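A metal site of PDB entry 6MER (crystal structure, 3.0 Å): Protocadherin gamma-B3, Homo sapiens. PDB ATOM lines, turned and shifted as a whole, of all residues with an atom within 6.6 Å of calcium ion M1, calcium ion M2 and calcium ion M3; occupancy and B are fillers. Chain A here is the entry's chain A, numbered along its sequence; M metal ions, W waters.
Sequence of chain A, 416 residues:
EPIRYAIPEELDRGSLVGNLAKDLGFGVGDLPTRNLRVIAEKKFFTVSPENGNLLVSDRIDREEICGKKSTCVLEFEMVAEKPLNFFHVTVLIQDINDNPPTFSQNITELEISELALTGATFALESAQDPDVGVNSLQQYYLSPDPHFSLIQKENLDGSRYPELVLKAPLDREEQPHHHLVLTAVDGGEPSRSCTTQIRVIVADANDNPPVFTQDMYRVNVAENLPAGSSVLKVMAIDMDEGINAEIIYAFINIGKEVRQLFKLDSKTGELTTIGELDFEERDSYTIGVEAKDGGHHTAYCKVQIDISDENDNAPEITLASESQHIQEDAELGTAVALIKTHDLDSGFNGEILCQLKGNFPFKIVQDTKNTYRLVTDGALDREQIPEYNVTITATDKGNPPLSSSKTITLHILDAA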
ATOM      1  N   GLU A 223      27.733 -11.967 -31.275  1.00  0.00           N
ATOM      2  CA  GLU A 223      28.909 -11.565 -32.048  1.00  0.00           C
ATOM      3  C   GLU A 223      30.209 -12.056 -31.431  1.00  0.00           C
ATOM      4  O   GLU A 223      31.211 -12.173 -32.140  1.00  0.00           O
ATOM      5  CB  GLU A 223      28.939 -10.042 -32.216  1.00  0.00           C
ATOM      6  CG  GLU A 223      28.825  -9.270 -30.919  1.00  0.00           C
ATOM      7  CD  GLU A 223      28.881  -7.776 -31.135  1.00  0.00           C
ATOM      8  OE1 GLU A 223      29.500  -7.339 -32.127  1.00  0.00           O
ATOM      9  OE2 GLU A 223      28.305  -7.033 -30.313  1.00  0.00           O
ATOM     10  N   LEU A 277      32.361 -12.787 -35.978  1.00  0.00           N
ATOM     11  CA  LEU A 277      31.120 -12.048 -36.121  1.00  0.00           C
ATOM     12  C   LEU A 277      31.233 -10.683 -35.460  1.00  0.00           C
ATOM     13  O   LEU A 277      31.902 -10.521 -34.441  1.00  0.00           O
ATOM     14  CB  LEU A 277      29.952 -12.834 -35.508  1.00  0.00           C
ATOM     15  CG  LEU A 277      29.560 -14.186 -36.115  1.00  0.00           C
ATOM     16  CD1 LEU A 277      29.623 -14.142 -37.644  1.00  0.00           C
ATOM     17  CD2 LEU A 277      30.418 -15.322 -35.568  1.00  0.00           C
ATOM     18  N   ASP A 278      30.559  -9.695 -36.058  1.00  0.00           N
ATOM     19  CA  ASP A 278      30.568  -8.329 -35.539  1.00  0.00           C
ATOM     20  C   ASP A 278      29.192  -7.723 -35.784  1.00  0.00           C
ATOM     21  O   ASP A 278      28.803  -7.527 -36.935  1.00  0.00           O
ATOM     22  CB  ASP A 278      31.667  -7.498 -36.193  1.00  0.00           C
ATOM     23  CG  ASP A 278      31.877  -6.168 -35.494  1.00  0.00           C
ATOM     24  OD1 ASP A 278      32.315  -6.163 -34.329  1.00  0.00           O
ATOM     25  OD2 ASP A 278      31.610  -5.121 -36.116  1.00  0.00           O
ATOM     26  N   PHE A 279      28.467  -7.437 -34.694  1.00  0.00           N
ATOM     27  CA  PHE A 279      27.152  -6.829 -34.827  1.00  0.00           C
ATOM     28  C   PHE A 279      27.233  -5.418 -35.410  1.00  0.00           C
ATOM     29  O   PHE A 279      26.280  -4.952 -36.038  1.00  0.00           O
ATOM     30  CB  PHE A 279      26.448  -6.809 -33.469  1.00  0.00           C
ATOM     31  CG  PHE A 279      25.059  -6.245 -33.507  1.00  0.00           C
ATOM     32  CD1 PHE A 279      23.994  -7.037 -33.878  1.00  0.00           C
ATOM     33  CD2 PHE A 279      24.824  -4.923 -33.160  1.00  0.00           C
ATOM     34  CE1 PHE A 279      22.701  -6.522 -33.908  1.00  0.00           C
ATOM     35  CE2 PHE A 279      23.543  -4.402 -33.186  1.00  0.00           C
ATOM     36  CZ  PHE A 279      22.486  -5.208 -33.562  1.00  0.00           C
ATOM     37  N   GLU A 280      28.364  -4.729 -35.193  1.00  0.00           N
ATOM     38  CA  GLU A 280      28.517  -3.384 -35.728  1.00  0.00           C
ATOM     39  C   GLU A 280      28.767  -3.369 -37.230  1.00  0.00           C
ATOM     40  O   GLU A 280      28.490  -2.355 -37.880  1.00  0.00           O
ATOM     41  CB  GLU A 280      29.650  -2.657 -34.997  1.00  0.00           C
ATOM     42  CG  GLU A 280      29.284  -2.150 -33.608  1.00  0.00           C
ATOM     43  CD  GLU A 280      29.027  -3.280 -32.621  1.00  0.00           C
ATOM     44  OE1 GLU A 280      29.596  -4.378 -32.803  1.00  0.00           O
ATOM     45  OE2 GLU A 280      28.262  -3.062 -31.661  1.00  0.00           O
ATOM     46  N   GLU A 281      29.280  -4.464 -37.792  1.00  0.00           N
ATOM     47  CA  GLU A 281      29.534  -4.539 -39.221  1.00  0.00           C
ATOM     48  C   GLU A 281      28.319  -5.062 -39.978  1.00  0.00           C
ATOM     49  O   GLU A 281      27.913  -4.469 -40.987  1.00  0.00           O
ATOM     50  CB  GLU A 281      30.750  -5.434 -39.487  1.00  0.00           C
ATOM     51  CG  GLU A 281      31.125  -5.565 -40.964  1.00  0.00           C
ATOM     52  CD  GLU A 281      31.735  -4.304 -41.538  1.00  0.00           C
ATOM     53  OE1 GLU A 281      32.119  -3.404 -40.753  1.00  0.00           O
ATOM     54  OE2 GLU A 281      31.825  -4.197 -42.774  1.00  0.00           O
ATOM     55  N   SER A 308      23.246 -11.115 -32.186  1.00  0.00           N
ATOM     56  CA  SER A 308      22.883 -10.293 -31.036  1.00  0.00           C
ATOM     57  C   SER A 308      24.017  -9.336 -30.687  1.00  0.00           C
ATOM     58  O   SER A 308      25.195  -9.650 -30.876  1.00  0.00           O
ATOM     59  CB  SER A 308      22.545 -11.175 -29.832  1.00  0.00           C
ATOM     60  OG  SER A 308      21.455 -12.030 -30.105  1.00  0.00           O
ATOM     61  N   ASP A 309      23.637  -8.173 -30.182  1.00  0.00           N
ATOM     62  CA  ASP A 309      24.610  -7.148 -29.817  1.00  0.00           C
ATOM     63  C   ASP A 309      25.218  -7.479 -28.450  1.00  0.00           C
ATOM     64  O   ASP A 309      24.492  -7.577 -27.456  1.00  0.00           O
ATOM     65  CB  ASP A 309      23.961  -5.768 -29.797  1.00  0.00           C
ATOM     66  CG  ASP A 309      24.945  -4.652 -29.532  1.00  0.00           C
ATOM     67  OD1 ASP A 309      26.163  -4.881 -29.697  1.00  0.00           O
ATOM     68  OD2 ASP A 309      24.504  -3.547 -29.157  1.00  0.00           O
ATOM     69  N   GLU A 310      26.535  -7.644 -28.416  1.00  0.00           N
ATOM     70  CA  GLU A 310      27.266  -7.825 -27.169  1.00  0.00           C
ATOM     71  C   GLU A 310      27.990  -6.534 -26.803  1.00  0.00           C
ATOM     72  O   GLU A 310      28.404  -5.768 -27.674  1.00  0.00           O
ATOM     73  CB  GLU A 310      28.262  -8.980 -27.287  1.00  0.00           C
ATOM     74  CG  GLU A 310      27.637 -10.358 -27.209  1.00  0.00           C
ATOM     75  CD  GLU A 310      27.154 -10.707 -25.820  1.00  0.00           C
ATOM     76  OE1 GLU A 310      27.573 -10.047 -24.849  1.00  0.00           O
ATOM     77  OE2 GLU A 310      26.345 -11.654 -25.687  1.00  0.00           O
ATOM     78  N   ASN A 311      28.145  -6.308 -25.504  1.00  0.00           N
ATOM     79  CA  ASN A 311      28.801  -5.110 -24.992  1.00  0.00           C
ATOM     80  C   ASN A 311      30.319  -5.285 -25.065  1.00  0.00           C
ATOM     81  O   ASN A 311      31.016  -5.454 -24.069  1.00  0.00           O
ATOM     82  CB  ASN A 311      28.343  -4.802 -23.579  1.00  0.00           C
ATOM     83  CG  ASN A 311      28.702  -3.405 -23.132  1.00  0.00           C
ATOM     84  OD1 ASN A 311      28.768  -2.477 -23.944  1.00  0.00           O
ATOM     85  ND2 ASN A 311      28.948  -3.227 -21.838  1.00  0.00           N
ATOM     86  N   ASP A 312      30.829  -5.241 -26.295  1.00  0.00           N
ATOM     87  CA  ASP A 312      32.251  -5.404 -26.567  1.00  0.00           C
ATOM     88  C   ASP A 312      32.923  -4.118 -27.013  1.00  0.00           C
ATOM     89  O   ASP A 312      34.056  -4.150 -27.505  1.00  0.00           O
ATOM     90  CB  ASP A 312      32.474  -6.512 -27.608  1.00  0.00           C
ATOM     91  CG  ASP A 312      31.682  -6.278 -28.884  1.00  0.00           C
ATOM     92  OD1 ASP A 312      30.961  -5.253 -28.964  1.00  0.00           O
ATOM     93  OD2 ASP A 312      31.779  -7.121 -29.798  1.00  0.00           O
ATOM     94  N   ASN A 313      32.248  -2.971 -26.865  1.00  0.00           N
ATOM     95  CA  ASN A 313      32.812  -1.681 -27.210  1.00  0.00           C
ATOM     96  C   ASN A 313      32.641  -0.726 -26.024  1.00  0.00           C
ATOM     97  O   ASN A 313      31.533  -0.601 -25.495  1.00  0.00           O
ATOM     98  CB  ASN A 313      32.152  -1.094 -28.462  1.00  0.00           C
ATOM     99  CG  ASN A 313      32.677  -1.727 -29.739  1.00  0.00           C
ATOM    100  OD1 ASN A 313      33.624  -1.230 -30.341  1.00  0.00           O
ATOM    101  ND2 ASN A 313      32.058  -2.817 -30.158  1.00  0.00           N
ATOM    102  N   ALA A 314      33.729  -0.082 -25.633  1.00  0.00           N
ATOM    103  CA  ALA A 314      33.684   0.865 -24.518  1.00  0.00           C
ATOM    104  C   ALA A 314      33.414   2.278 -25.028  1.00  0.00           C
ATOM    105  O   ALA A 314      33.872   2.646 -26.119  1.00  0.00           O
ATOM    106  CB  ALA A 314      34.999   0.847 -23.748  1.00  0.00           C
ATOM    107  N   PRO A 315      32.669   3.082 -24.269  1.00  0.00           N
ATOM    108  CA  PRO A 315      32.381   4.459 -24.697  1.00  0.00           C
ATOM    109  C   PRO A 315      33.654   5.301 -24.682  1.00  0.00           C
ATOM    110  O   PRO A 315      34.320   5.421 -23.663  1.00  0.00           O
ATOM    111  CB  PRO A 315      31.369   4.953 -23.660  1.00  0.00           C
ATOM    112  CG  PRO A 315      30.838   3.716 -22.994  1.00  0.00           C
ATOM    113  CD  PRO A 315      31.975   2.734 -23.020  1.00  0.00           C
ATOM    114  N   ASP A 343      28.924   5.374 -28.224  1.00  0.00           N
ATOM    115  CA  ASP A 343      29.234   3.959 -28.077  1.00  0.00           C
ATOM    116  C   ASP A 343      28.764   3.226 -29.326  1.00  0.00           C
ATOM    117  O   ASP A 343      27.612   3.399 -29.755  1.00  0.00           O
ATOM    118  CB  ASP A 343      28.579   3.377 -26.832  1.00  0.00           C
ATOM    119  CG  ASP A 343      29.145   2.032 -26.449  1.00  0.00           C
ATOM    120  OD1 ASP A 343      30.156   1.993 -25.714  1.00  0.00           O
ATOM    121  OD2 ASP A 343      28.589   1.001 -26.883  1.00  0.00           O
ATOM    122  N   LEU A 344      29.648   2.421 -29.918  1.00  0.00           N
ATOM    123  CA  LEU A 344      29.328   1.746 -31.169  1.00  0.00           C
ATOM    124  C   LEU A 344      28.217   0.710 -31.006  1.00  0.00           C
ATOM    125  O   LEU A 344      27.546   0.390 -31.989  1.00  0.00           O
ATOM    126  CB  LEU A 344      30.575   1.079 -31.738  1.00  0.00           C
ATOM    127  CG  LEU A 344      31.767   2.000 -32.025  1.00  0.00           C
ATOM    128  CD1 LEU A 344      32.890   1.227 -32.700  1.00  0.00           C
ATOM    129  CD2 LEU A 344      31.332   3.194 -32.869  1.00  0.00           C
ATOM    130  N   ASP A 345      28.004   0.203 -29.798  1.00  0.00           N
ATOM    131  CA  ASP A 345      26.964  -0.779 -29.578  1.00  0.00           C
ATOM    132  C   ASP A 345      25.584  -0.123 -29.639  1.00  0.00           C
ATOM    133  O   ASP A 345      25.439   1.105 -29.541  1.00  0.00           O
ATOM    134  CB  ASP A 345      27.143  -1.470 -28.227  1.00  0.00           C
ATOM    135  CG  ASP A 345      28.547  -1.973 -28.013  1.00  0.00           C
ATOM    136  OD1 ASP A 345      29.188  -2.396 -29.006  1.00  0.00           O
ATOM    137  OD2 ASP A 345      29.029  -1.955 -26.857  1.00  0.00           O
ATOM    138  N   SER A 346      24.565  -0.952 -29.825  1.00  0.00           N
ATOM    139  CA  SER A 346      23.184  -0.495 -29.905  1.00  0.00           C
ATOM    140  C   SER A 346      22.440  -0.815 -28.606  1.00  0.00           C
ATOM    141  O   SER A 346      22.968  -1.472 -27.698  1.00  0.00           O
ATOM    142  CB  SER A 346      22.474  -1.133 -31.098  1.00  0.00           C
ATOM    143  OG  SER A 346      23.142  -0.835 -32.309  1.00  0.00           O
ATOM    144  N   PHE A 348      20.698  -0.521 -24.972  1.00  0.00           N
ATOM    145  CA  PHE A 348      21.227   0.015 -23.719  1.00  0.00           C
ATOM    146  C   PHE A 348      22.743  -0.138 -23.633  1.00  0.00           C
ATOM    147  O   PHE A 348      23.369   0.538 -22.808  1.00  0.00           O
ATOM    148  CB  PHE A 348      20.563  -0.669 -22.525  1.00  0.00           C
ATOM    149  CG  PHE A 348      19.208  -0.123 -22.197  1.00  0.00           C
ATOM    150  CD1 PHE A 348      19.076   1.003 -21.394  1.00  0.00           C
ATOM    151  CD2 PHE A 348      18.056  -0.721 -22.684  1.00  0.00           C
ATOM    152  CE1 PHE A 348      17.839   1.520 -21.088  1.00  0.00           C
ATOM    153  CE2 PHE A 348      16.807  -0.210 -22.382  1.00  0.00           C
ATOM    154  CZ  PHE A 348      16.695   0.907 -21.579  1.00  0.00           C
ATOM    155  N   ASN A 349      23.335  -1.007 -24.455  1.00  0.00           N
ATOM    156  CA  ASN A 349      24.791  -1.088 -24.504  1.00  0.00           C
ATOM    157  C   ASN A 349      25.417   0.165 -25.092  1.00  0.00           C
ATOM    158  O   ASN A 349      26.615   0.397 -24.901  1.00  0.00           O
ATOM    159  CB  ASN A 349      25.219  -2.305 -25.330  1.00  0.00           C
ATOM    160  CG  ASN A 349      24.649  -3.609 -24.794  1.00  0.00           C
ATOM    161  OD1 ASN A 349      24.616  -3.831 -23.590  1.00  0.00           O
ATOM    162  ND2 ASN A 349      24.190  -4.462 -25.700  1.00  0.00           N
ATOM    163  N   GLY A 350      24.630   0.990 -25.785  1.00  0.00           N
ATOM    164  CA  GLY A 350      25.140   2.199 -26.405  1.00  0.00           C
ATOM    165  C   GLY A 350      24.830   3.459 -25.623  1.00  0.00           C
ATOM    166  O   GLY A 350      25.490   4.481 -25.804  1.00  0.00           O
ATOM    167  N   GLU A 351      23.833   3.402 -24.738  1.00  0.00           N
ATOM    168  CA  GLU A 351      23.523   4.541 -23.897  1.00  0.00           C
ATOM    169  C   GLU A 351      24.636   4.771 -22.879  1.00  0.00           C
ATOM    170  O   GLU A 351      25.130   3.826 -22.266  1.00  0.00           O
ATOM    171  CB  GLU A 351      22.182   4.351 -23.186  1.00  0.00           C
ATOM    172  CG  GLU A 351      20.981   4.397 -24.120  1.00  0.00           C
ATOM    173  CD  GLU A 351      19.668   4.496 -23.362  1.00  0.00           C
ATOM    174  OE1 GLU A 351      19.699   4.612 -22.123  1.00  0.00           O
ATOM    175  OE2 GLU A 351      18.595   4.474 -24.013  1.00  0.00           O
ATOM    176  N   ASP A 396      28.764   2.963 -19.879  1.00  0.00           N
ATOM    177  CA  ASP A 396      27.550   2.556 -20.582  1.00  0.00           C
ATOM    178  C   ASP A 396      26.608   1.820 -19.638  1.00  0.00           C
ATOM    179  O   ASP A 396      26.947   1.503 -18.493  1.00  0.00           O
ATOM    180  CB  ASP A 396      27.905   1.697 -21.791  1.00  0.00           C
ATOM    181  CG  ASP A 396      28.768   0.487 -21.443  1.00  0.00           C
ATOM    182  OD1 ASP A 396      28.905   0.173 -20.245  1.00  0.00           O
ATOM    183  OD2 ASP A 396      29.312  -0.127 -22.372  1.00  0.00           O
ATOM    184  N   LYS A 397      25.397   1.550 -20.135  1.00  0.00           N
ATOM    185  CA  LYS A 397      24.369   0.883 -19.346  1.00  0.00           C
ATOM    186  C   LYS A 397      24.192  -0.580 -19.735  1.00  0.00           C
ATOM    187  O   LYS A 397      23.109  -1.148 -19.567  1.00  0.00           O
ATOM    188  CB  LYS A 397      23.037   1.627 -19.493  1.00  0.00           C
ATOM    189  CG  LYS A 397      23.105   3.080 -19.033  1.00  0.00           C
ATOM    190  CD  LYS A 397      21.760   3.769 -19.214  1.00  0.00           C
ATOM    191  CE  LYS A 397      21.831   5.220 -18.763  1.00  0.00           C
ATOM    192  NZ  LYS A 397      20.513   5.903 -18.908  1.00  0.00           N
ATOM    193  N   GLY A 398      25.247  -1.207 -20.268  1.00  0.00           N
ATOM    194  CA  GLY A 398      25.190  -2.592 -20.678  1.00  0.00           C
ATOM    195  C   GLY A 398      25.479  -3.556 -19.547  1.00  0.00           C
ATOM    196  O   GLY A 398      25.559  -3.186 -18.377  1.00  0.00           O
ATOM    197  N   LEU A 402      30.903  -1.295 -19.349  1.00  0.00           N
ATOM    198  CA  LEU A 402      32.258  -0.868 -19.646  1.00  0.00           C
ATOM    199  C   LEU A 402      32.349   0.658 -19.534  1.00  0.00           C
ATOM    200  O   LEU A 402      31.350   1.364 -19.672  1.00  0.00           O
ATOM    201  CB  LEU A 402      32.700  -1.309 -21.047  1.00  0.00           C
ATOM    202  CG  LEU A 402      32.730  -2.817 -21.296  1.00  0.00           C
ATOM    203  CD1 LEU A 402      33.165  -3.119 -22.730  1.00  0.00           C
ATOM    204  CD2 LEU A 402      33.661  -3.508 -20.307  1.00  0.00           C
HETATM  205 CA    CA M   1      29.196  -0.234 -24.887  1.00  0.00          CA
HETATM  206 CA    CA M   2      28.719  -4.659 -29.894  1.00  0.00          CA
HETATM  207 CA    CA M   3      31.506  -5.783 -31.949  1.00  0.00          CA
HETATM  208  O   HOH W   1      32.792  -7.972 -32.301  1.00  0.00           O
HETATM  209  O   HOH W   2      34.506  -4.845 -30.858  1.00  0.00           O
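Calcium ion M3 is bound by OE1 of Glu 280 (2.5 Å), OD1 of Asp 278 (2.5 Å), OE1 of Glu 223 (2.5 Å), OD2 of Asp 312 (2.5 Å) and water W1 (2.6 Å). Slightly farther from calcium ion M3 lies the side-chain carboxylate (OD1) of Asp 312 (3.1 Å).
Calcium ion M2 is bound by OE2 of Glu 280 (2.4 Å), OE2 of Glu 223 (2.4 Å), OD1 of Asp 345 (2.5 Å), OD1 of Asp 312 (2.5 Å), O of Glu 310 (2.5 Å) and OD1 of Asp 309 (2.6 Å). Calcium ion M2 has six donor atoms within binding distance. Slightly farther from calcium ion M2 lies OE1 of Glu 280 (3.1 Å).
Water W2 lies within hydrogen-bond range of ND2 of Asn 313 and O of Asp 312.
Six residues have an atom within 4 Å of calcium ion M1: Asn 311, Asn 313, Asp 343, Asp 345, Asn 349 and Asp 396. Along chain A the residues within 4 Å of calcium ion M1 span positions 311 to 396.
OD2 of Asp 343 is bound to calcium ion M1 (2.4 Å). O of Asn 313 binds calcium ion M1 (2.4 Å). OD1 of Asn 311 is bound to calcium ion M1 (2.5 Å). The side-chain carboxylate (OD2) of Asp 396 binds calcium ion M1, 2.5 Å away. OD1 of Asp 343 binds calcium ion M1 (2.6 Å). The side-chain carboxylate (OD2) of Asp 345 binds calcium ion M1 (2.6 Å). Calcium ion M1 is bound by the backbone carbonyl oxygen (O) of Asn 349, at 2.7 Å.
The side-chain amide nitrogen (ND2) of Asn 313 lies close to the side-chain carboxylate (OD1) of Asp 312 (2.9 Å). The side-chain carboxylate of Glu 223 sits close to the backbone NH of Phe 279, at 2.8 Å. The backbone carbonyl oxygen of Ser 308 is in hydrogen-bond range of the backbone NH of Glu 223. The backbone NH of Leu 402 lies within hydrogen-bond range of the side-chain carboxylate of Asp 396, at 2.6 Å. The backbone NH (N) of Glu 281 is in hydrogen-bond range of the side-chain carboxylate (OD2) of Asp 278 (2.9 Å). N of Ser 346 sits at hydrogen-bond distance from OD2 of Asp 309, 2.7 Å away.
Seven residues have an atom within 4 Å of calcium ion M2: Glu 223, Glu 280, Asp 309, Glu 310, Asp 312, Asn 313 and Asp 345.
Five residues have an atom within 4 Å of calcium ion M3: Glu 223, Asp 278, Glu 280, Asp 312 and Asn 313. Along chain A the residues within 4 Å of calcium ion M3 span positions 223 to 313.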
